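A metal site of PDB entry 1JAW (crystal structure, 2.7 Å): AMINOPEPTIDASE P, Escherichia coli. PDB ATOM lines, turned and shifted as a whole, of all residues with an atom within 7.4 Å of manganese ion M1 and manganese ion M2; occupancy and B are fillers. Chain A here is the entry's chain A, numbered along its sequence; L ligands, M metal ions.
Manganese ion M1 is bound by OE1 of Glu 406, OD2 of Asp 260, O1 of the ligand, OD1 of Asp 260 and OD1 of Asp 271. Manganese ion M1 has five donor atoms within binding distance.
Tyr 229 touches manganese ion M1. Thr 273 touches manganese ion M1 (OG1 to MN, 3.5 Å). The nearest printed residue that does not touch manganese ion M1 is Glu 383 (4.03 Å).
Manganese ion M2 is bound by NE2 of His 354 (2.0 Å), O1 of the ligand (2.2 Å), OD2 of Asp 271 (2.2 Å), OE2 of Glu 406 (2.3 Å) and OE2 of Glu 383 (2.5 Å). Manganese ion M2 has five donor atoms within binding distance. Slightly farther from manganese ion M2 lies OE1 of Glu 406 (2.9 Å).
CG2 of Thr 381 touches manganese ion M2, 3.8 Å away. Within 4 Å of manganese ion M2: Asp 271, His 354, Thr 381, Glu 383 and Glu 406.
The side-chain carboxylate of Glu 406 lies close to the side-chain hydroxyl of Thr 381 (3.5 Å). N of Ala 261 sits close to OH of Tyr 229, 3.0 Å away. The backbone carbonyl oxygen (O) of Val 360 lies within hydrogen-bond range of a ring nitrogen (ND1) of His 354, at 3.0 Å. NH2 of Arg 404 lies close to OD2 of Asp 260 (3.4 Å). OG of Ser 353 is in hydrogen-bond range of O of Thr 381, at 2.7 Å. The backbone NH (N) of Thr 381 sits at hydrogen-bond distance from the backbone carbonyl oxygen (O) of His 354, 2.6 Å away. The guanidinium group (NE) of Arg 404 sits at hydrogen-bond distance from the side-chain hydroxyl (OG1) of Thr 273, at 3.4 Å. The side-chain carboxylate (OD1) of Asp 271 sits close to the side-chain hydroxyl (OH) of Tyr 229 (2.7 Å).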
ATOM      1  N   TYR A 229      14.101 -11.120  18.287  1.00  0.00           N
ATOM      2  CA  TYR A 229      14.413  -9.700  18.110  1.00  0.00           C
ATOM      3  C   TYR A 229      14.797  -9.155  19.482  1.00  0.00           C
ATOM      4  O   TYR A 229      14.562  -9.806  20.509  1.00  0.00           O
ATOM      5  CB  TYR A 229      13.198  -8.914  17.577  1.00  0.00           C
ATOM      6  CG  TYR A 229      11.952  -9.071  18.419  1.00  0.00           C
ATOM      7  CD1 TYR A 229      11.083 -10.127  18.204  1.00  0.00           C
ATOM      8  CD2 TYR A 229      11.657  -8.187  19.466  1.00  0.00           C
ATOM      9  CE1 TYR A 229       9.960 -10.330  18.985  1.00  0.00           C
ATOM     10  CE2 TYR A 229      10.525  -8.385  20.271  1.00  0.00           C
ATOM     11  CZ  TYR A 229       9.689  -9.454  20.016  1.00  0.00           C
ATOM     12  OH  TYR A 229       8.566  -9.667  20.778  1.00  0.00           O
ATOM     13  N   ILE A 232      12.113  -5.415  24.297  1.00  0.00           N
ATOM     14  CA  ILE A 232      11.677  -4.081  24.691  1.00  0.00           C
ATOM     15  C   ILE A 232      11.093  -4.129  26.100  1.00  0.00           C
ATOM     16  O   ILE A 232      10.175  -4.922  26.362  1.00  0.00           O
ATOM     17  CB  ILE A 232      10.529  -3.546  23.790  1.00  0.00           C
ATOM     18  CG1 ILE A 232      10.791  -3.770  22.300  1.00  0.00           C
ATOM     19  CG2 ILE A 232      10.303  -2.079  24.071  1.00  0.00           C
ATOM     20  CD1 ILE A 232      11.896  -2.941  21.742  1.00  0.00           C
ATOM     21  N   HIS A 243      10.421   0.976  19.769  1.00  0.00           N
ATOM     22  CA  HIS A 243      11.474  -0.006  19.960  1.00  0.00           C
ATOM     23  C   HIS A 243      12.507   0.570  20.950  1.00  0.00           C
ATOM     24  O   HIS A 243      13.583   1.033  20.573  1.00  0.00           O
ATOM     25  CB  HIS A 243      12.144  -0.408  18.614  1.00  0.00           C
ATOM     26  CG  HIS A 243      11.216  -1.047  17.623  1.00  0.00           C
ATOM     27  ND1 HIS A 243      11.369  -0.876  16.260  1.00  0.00           N
ATOM     28  CD2 HIS A 243      10.151  -1.866  17.772  1.00  0.00           C
ATOM     29  CE1 HIS A 243      10.425  -1.554  15.620  1.00  0.00           C
ATOM     30  NE2 HIS A 243       9.672  -2.171  16.518  1.00  0.00           N
ATOM     31  N   ILE A 259       6.303  -4.609  27.742  1.00  0.00           N
ATOM     32  CA  ILE A 259       7.286  -5.613  27.361  1.00  0.00           C
ATOM     33  C   ILE A 259       7.004  -6.186  25.974  1.00  0.00           C
ATOM     34  O   ILE A 259       5.972  -6.825  25.773  1.00  0.00           O
ATOM     35  CB  ILE A 259       7.339  -6.757  28.368  1.00  0.00           C
ATOM     36  CG1 ILE A 259       7.691  -6.212  29.759  1.00  0.00           C
ATOM     37  CG2 ILE A 259       8.336  -7.796  27.923  1.00  0.00           C
ATOM     38  CD1 ILE A 259       7.892  -7.262  30.798  1.00  0.00           C
ATOM     39  N   ASP A 260       8.044  -5.890  24.987  1.00  0.00           N
ATOM     40  CA  ASP A 260       7.716  -6.453  23.706  1.00  0.00           C
ATOM     41  C   ASP A 260       9.049  -7.684  23.458  1.00  0.00           C
ATOM     42  O   ASP A 260      10.098  -7.225  23.506  1.00  0.00           O
ATOM     43  CB  ASP A 260       7.597  -5.654  22.596  1.00  0.00           C
ATOM     44  CG  ASP A 260       7.109  -6.273  21.323  1.00  0.00           C
ATOM     45  OD1 ASP A 260       6.737  -7.476  21.276  1.00  0.00           O
ATOM     46  OD2 ASP A 260       7.109  -5.676  20.273  1.00  0.00           O
ATOM     47  N   ALA A 261       8.705  -8.830  23.679  1.00  0.00           N
ATOM     48  CA  ALA A 261       9.719  -9.880  23.659  1.00  0.00           C
ATOM     49  C   ALA A 261       9.213 -11.170  23.021  1.00  0.00           C
ATOM     50  O   ALA A 261       8.070 -11.592  23.246  1.00  0.00           O
ATOM     51  CB  ALA A 261      10.227 -10.153  25.067  1.00  0.00           C
ATOM     52  N   GLY A 262      10.073 -11.790  22.197  1.00  0.00           N
ATOM     53  CA  GLY A 262       9.724 -13.035  21.522  1.00  0.00           C
ATOM     54  C   GLY A 262      10.884 -14.005  21.390  1.00  0.00           C
ATOM     55  O   GLY A 262      12.027 -13.606  21.157  1.00  0.00           O
ATOM     56  N   GLY A 270       8.488 -15.804  17.962  1.00  0.00           N
ATOM     57  CA  GLY A 270       7.362 -15.647  18.854  1.00  0.00           C
ATOM     58  C   GLY A 270       7.193 -14.156  19.127  1.00  0.00           C
ATOM     59  O   GLY A 270       8.122 -13.360  18.904  1.00  0.00           O
ATOM     60  N   ASP A 271       5.855 -13.259  19.181  1.00  0.00           N
ATOM     61  CA  ASP A 271       5.764 -11.627  19.230  1.00  0.00           C
ATOM     62  C   ASP A 271       4.890 -11.539  20.174  1.00  0.00           C
ATOM     63  O   ASP A 271       3.740 -11.548  19.807  1.00  0.00           O
ATOM     64  CB  ASP A 271       5.429 -11.231  17.980  1.00  0.00           C
ATOM     65  CG  ASP A 271       6.197 -10.051  17.784  1.00  0.00           C
ATOM     66  OD1 ASP A 271       6.704  -9.593  18.838  1.00  0.00           O
ATOM     67  OD2 ASP A 271       6.220  -9.298  16.597  1.00  0.00           O
ATOM     68  N   ILE A 272       5.377 -11.257  21.335  1.00  0.00           N
ATOM     69  CA  ILE A 272       4.309 -10.924  22.266  1.00  0.00           C
ATOM     70  C   ILE A 272       4.555  -9.604  22.973  1.00  0.00           C
ATOM     71  O   ILE A 272       5.675  -9.281  23.358  1.00  0.00           O
ATOM     72  CB  ILE A 272       4.168 -12.009  23.373  1.00  0.00           C
ATOM     73  CG1 ILE A 272       3.456 -13.274  22.843  1.00  0.00           C
ATOM     74  CG2 ILE A 272       3.350 -11.498  24.541  1.00  0.00           C
ATOM     75  CD1 ILE A 272       3.123 -14.281  23.944  1.00  0.00           C
ATOM     76  N   THR A 273       3.493  -8.810  23.116  1.00  0.00           N
ATOM     77  CA  THR A 273       3.580  -7.547  23.831  1.00  0.00           C
ATOM     78  C   THR A 273       2.519  -7.531  24.928  1.00  0.00           C
ATOM     79  O   THR A 273       1.370  -7.885  24.689  1.00  0.00           O
ATOM     80  CB  THR A 273       3.366  -6.302  22.952  1.00  0.00           C
ATOM     81  OG1 THR A 273       4.194  -6.379  21.791  1.00  0.00           O
ATOM     82  CG2 THR A 273       3.749  -5.055  23.732  1.00  0.00           C
ATOM     83  N   LEU A 352      -1.125  -2.498  12.330  1.00  0.00           N
ATOM     84  CA  LEU A 352      -1.832  -3.341  13.289  1.00  0.00           C
ATOM     85  C   LEU A 352      -1.310  -4.780  13.267  1.00  0.00           C
ATOM     86  O   LEU A 352      -1.365  -5.504  14.272  1.00  0.00           O
ATOM     87  CB  LEU A 352      -3.347  -3.340  12.970  1.00  0.00           C
ATOM     88  CG  LEU A 352      -4.240  -4.235  13.830  1.00  0.00           C
ATOM     89  CD1 LEU A 352      -4.432  -3.608  15.187  1.00  0.00           C
ATOM     90  CD2 LEU A 352      -5.575  -4.459  13.160  1.00  0.00           C
ATOM     91  N   SER A 353      -0.791  -5.189  12.120  1.00  0.00           N
ATOM     92  CA  SER A 353      -0.294  -6.536  11.950  1.00  0.00           C
ATOM     93  C   SER A 353       0.909  -6.604  11.017  1.00  0.00           C
ATOM     94  O   SER A 353       0.841  -6.209   9.849  1.00  0.00           O
ATOM     95  CB  SER A 353      -1.423  -7.413  11.403  1.00  0.00           C
ATOM     96  OG  SER A 353      -2.500  -7.452  12.312  1.00  0.00           O
ATOM     97  N   HIS A 354       1.893  -7.656  11.380  1.00  0.00           N
ATOM     98  CA  HIS A 354       2.919  -8.009  10.358  1.00  0.00           C
ATOM     99  C   HIS A 354       2.814  -9.663  10.355  1.00  0.00           C
ATOM    100  O   HIS A 354       2.243 -10.299  11.453  1.00  0.00           O
ATOM    101  CB  HIS A 354       4.317  -7.429  10.672  1.00  0.00           C
ATOM    102  CG  HIS A 354       4.698  -7.771  12.050  1.00  0.00           C
ATOM    103  ND1 HIS A 354       5.250  -9.003  12.374  1.00  0.00           N
ATOM    104  CD2 HIS A 354       4.707  -7.145  13.257  1.00  0.00           C
ATOM    105  CE1 HIS A 354       5.593  -9.008  13.718  1.00  0.00           C
ATOM    106  NE2 HIS A 354       5.317  -7.856  14.399  1.00  0.00           N
ATOM    107  N   TRP A 355       3.202 -10.044   8.992  1.00  0.00           N
ATOM    108  CA  TRP A 355       3.448 -11.470   8.815  1.00  0.00           C
ATOM    109  C   TRP A 355       4.436 -11.966   9.873  1.00  0.00           C
ATOM    110  O   TRP A 355       5.328 -11.232  10.291  1.00  0.00           O
ATOM    111  CB  TRP A 355       4.030 -11.759   7.431  1.00  0.00           C
ATOM    112  CG  TRP A 355       3.226 -11.265   6.250  1.00  0.00           C
ATOM    113  CD1 TRP A 355       3.723 -10.654   5.143  1.00  0.00           C
ATOM    114  CD2 TRP A 355       1.821 -11.415   6.030  1.00  0.00           C
ATOM    115  NE1 TRP A 355       2.721 -10.416   4.230  1.00  0.00           N
ATOM    116  CE2 TRP A 355       1.533 -10.879   4.753  1.00  0.00           C
ATOM    117  CE3 TRP A 355       0.765 -11.955   6.785  1.00  0.00           C
ATOM    118  CZ2 TRP A 355       0.236 -10.874   4.206  1.00  0.00           C
ATOM    119  CZ3 TRP A 355      -0.532 -11.949   6.238  1.00  0.00           C
ATOM    120  CH2 TRP A 355      -0.777 -11.398   4.969  1.00  0.00           C
ATOM    121  N   LEU A 356       4.294 -13.233  10.258  1.00  0.00           N
ATOM    122  CA  LEU A 356       5.168 -13.847  11.265  1.00  0.00           C
ATOM    123  C   LEU A 356       5.649 -15.229  10.800  1.00  0.00           C
ATOM    124  O   LEU A 356       4.859 -16.032  10.287  1.00  0.00           O
ATOM    125  CB  LEU A 356       4.411 -13.999  12.586  1.00  0.00           C
ATOM    126  CG  LEU A 356       5.166 -14.469  13.820  1.00  0.00           C
ATOM    127  CD1 LEU A 356       6.152 -13.407  14.315  1.00  0.00           C
ATOM    128  CD2 LEU A 356       4.168 -14.818  14.895  1.00  0.00           C
ATOM    129  N   VAL A 360      10.641 -12.342  12.469  1.00  0.00           N
ATOM    130  CA  VAL A 360       9.503 -11.689  13.169  1.00  0.00           C
ATOM    131  C   VAL A 360       8.673 -10.916  12.165  1.00  0.00           C
ATOM    132  O   VAL A 360       7.450 -11.048  12.143  1.00  0.00           O
ATOM    133  CB  VAL A 360       9.907 -10.652  14.214  1.00  0.00           C
ATOM    134  CG1 VAL A 360       9.588 -11.170  15.585  1.00  0.00           C
ATOM    135  CG2 VAL A 360      11.347 -10.224  14.063  1.00  0.00           C
ATOM    136  N   HIS A 361       9.337 -10.057  11.404  1.00  0.00           N
ATOM    137  CA  HIS A 361       8.678  -9.301  10.354  1.00  0.00           C
ATOM    138  C   HIS A 361       8.957 -10.157   9.132  1.00  0.00           C
ATOM    139  O   HIS A 361       9.898  -9.918   8.366  1.00  0.00           O
ATOM    140  CB  HIS A 361       9.287  -7.907  10.222  1.00  0.00           C
ATOM    141  CG  HIS A 361       9.134  -7.066  11.453  1.00  0.00           C
ATOM    142  ND1 HIS A 361       9.940  -5.982  11.725  1.00  0.00           N
ATOM    143  CD2 HIS A 361       8.288  -7.184  12.514  1.00  0.00           C
ATOM    144  CE1 HIS A 361       9.600  -5.472  12.895  1.00  0.00           C
ATOM    145  NE2 HIS A 361       8.606  -6.178  13.399  1.00  0.00           N
ATOM    146  N   THR A 381       0.775 -11.096  13.454  1.00  0.00           N
ATOM    147  CA  THR A 381       0.669 -10.544  14.805  1.00  0.00           C
ATOM    148  C   THR A 381      -0.570  -9.640  14.830  1.00  0.00           C
ATOM    149  O   THR A 381      -1.055  -9.214  13.785  1.00  0.00           O
ATOM    150  CB  THR A 381       1.890  -9.677  15.160  1.00  0.00           C
ATOM    151  OG1 THR A 381       1.909  -8.523  14.309  1.00  0.00           O
ATOM    152  CG2 THR A 381       3.173 -10.468  14.976  1.00  0.00           C
ATOM    153  N   VAL A 382      -1.101  -9.374  16.025  1.00  0.00           N
ATOM    154  CA  VAL A 382      -2.259  -8.488  16.176  1.00  0.00           C
ATOM    155  C   VAL A 382      -1.987  -7.456  17.269  1.00  0.00           C
ATOM    156  O   VAL A 382      -1.724  -7.796  18.418  1.00  0.00           O
ATOM    157  CB  VAL A 382      -3.549  -9.244  16.558  1.00  0.00           C
ATOM    158  CG1 VAL A 382      -4.720  -8.262  16.609  1.00  0.00           C
ATOM    159  CG2 VAL A 382      -3.848 -10.359  15.554  1.00  0.00           C
ATOM    160  N   GLU A 383      -1.397  -6.412  16.729  1.00  0.00           N
ATOM    161  CA  GLU A 383      -0.772  -5.575  17.879  1.00  0.00           C
ATOM    162  C   GLU A 383      -1.145  -3.981  17.907  1.00  0.00           C
ATOM    163  O   GLU A 383      -0.131  -2.916  17.403  1.00  0.00           O
ATOM    164  CB  GLU A 383       0.707  -5.647  17.735  1.00  0.00           C
ATOM    165  CG  GLU A 383       1.287  -5.407  16.434  1.00  0.00           C
ATOM    166  CD  GLU A 383       2.728  -5.451  16.381  1.00  0.00           C
ATOM    167  OE1 GLU A 383       3.403  -5.016  17.296  1.00  0.00           O
ATOM    168  OE2 GLU A 383       3.240  -6.068  15.393  1.00  0.00           O
ATOM    169  N   ARG A 404       0.761  -1.319  24.503  1.00  0.00           N
ATOM    170  CA  ARG A 404       0.631  -2.219  23.357  1.00  0.00           C
ATOM    171  C   ARG A 404       0.269  -3.594  23.909  1.00  0.00           C
ATOM    172  O   ARG A 404       0.702  -3.961  24.993  1.00  0.00           O
ATOM    173  CB  ARG A 404       1.930  -2.268  22.521  1.00  0.00           C
ATOM    174  CG  ARG A 404       1.865  -3.152  21.261  1.00  0.00           C
ATOM    175  CD  ARG A 404       2.981  -2.852  20.253  1.00  0.00           C
ATOM    176  NE  ARG A 404       4.342  -3.123  20.756  1.00  0.00           N
ATOM    177  CZ  ARG A 404       5.251  -2.188  21.035  1.00  0.00           C
ATOM    178  NH1 ARG A 404       4.971  -0.902  20.880  1.00  0.00           N
ATOM    179  NH2 ARG A 404       6.462  -2.536  21.432  1.00  0.00           N
ATOM    180  N   GLU A 406       0.118  -7.323  22.019  1.00  0.00           N
ATOM    181  CA  GLU A 406       0.379  -7.943  20.695  1.00  0.00           C
ATOM    182  C   GLU A 406       0.152  -9.624  20.937  1.00  0.00           C
ATOM    183  O   GLU A 406       0.493 -10.047  21.969  1.00  0.00           O
ATOM    184  CB  GLU A 406       1.793  -7.681  20.327  1.00  0.00           C
ATOM    185  CG  GLU A 406       2.329  -8.579  19.767  1.00  0.00           C
ATOM    186  CD  GLU A 406       3.314  -8.144  18.855  1.00  0.00           C
ATOM    187  OE1 GLU A 406       4.515  -7.472  19.246  1.00  0.00           O
ATOM    188  OE2 GLU A 406       3.294  -8.358  17.474  1.00  0.00           O
ATOM    189  N   ASP A 407      -0.549 -10.224  20.389  1.00  0.00           N
ATOM    190  CA  ASP A 407      -0.845 -11.625  20.142  1.00  0.00           C
ATOM    191  C   ASP A 407      -0.476 -12.074  18.739  1.00  0.00           C
ATOM    192  O   ASP A 407      -0.491 -11.292  17.789  1.00  0.00           O
ATOM    193  CB  ASP A 407      -2.323 -11.920  20.406  1.00  0.00           C
ATOM    194  CG  ASP A 407      -2.633 -12.177  21.874  1.00  0.00           C
ATOM    195  OD1 ASP A 407      -1.703 -12.144  22.706  1.00  0.00           O
ATOM    196  OD2 ASP A 407      -3.818 -12.418  22.186  1.00  0.00           O
ATOM    197  N   ASP A 408      -0.142 -13.363  18.608  1.00  0.00           N
ATOM    198  CA  ASP A 408       0.236 -13.948  17.331  1.00  0.00           C
ATOM    199  C   ASP A 408      -0.866 -14.914  16.942  1.00  0.00           C
ATOM    200  O   ASP A 408      -1.330 -15.698  17.775  1.00  0.00           O
ATOM    201  CB  ASP A 408       1.562 -14.700  17.454  1.00  0.00           C
ATOM    202  CG  ASP A 408       2.636 -13.868  18.115  1.00  0.00           C
ATOM    203  OD1 ASP A 408       2.706 -12.636  17.889  1.00  0.00           O
ATOM    204  OD2 ASP A 408       3.424 -14.459  18.883  1.00  0.00           O
HETATM  205  C1  LIG L   1       7.822  -6.062  17.120  1.00  0.00           C
HETATM  206  O1  LIG L   1       6.593  -6.093  17.132  1.00  0.00           O
HETATM  207  O2  LIG L   1       8.203  -6.008  15.934  1.00  0.00           O
HETATM  208  C2  LIG L   1       8.793  -6.158  18.110  1.00  0.00           C
HETATM  209 MN    MN M   1       6.255  -7.251  19.052  1.00  0.00          MN
HETATM  210 MN    MN M   2       5.074  -7.454  16.366  1.00  0.00          MN
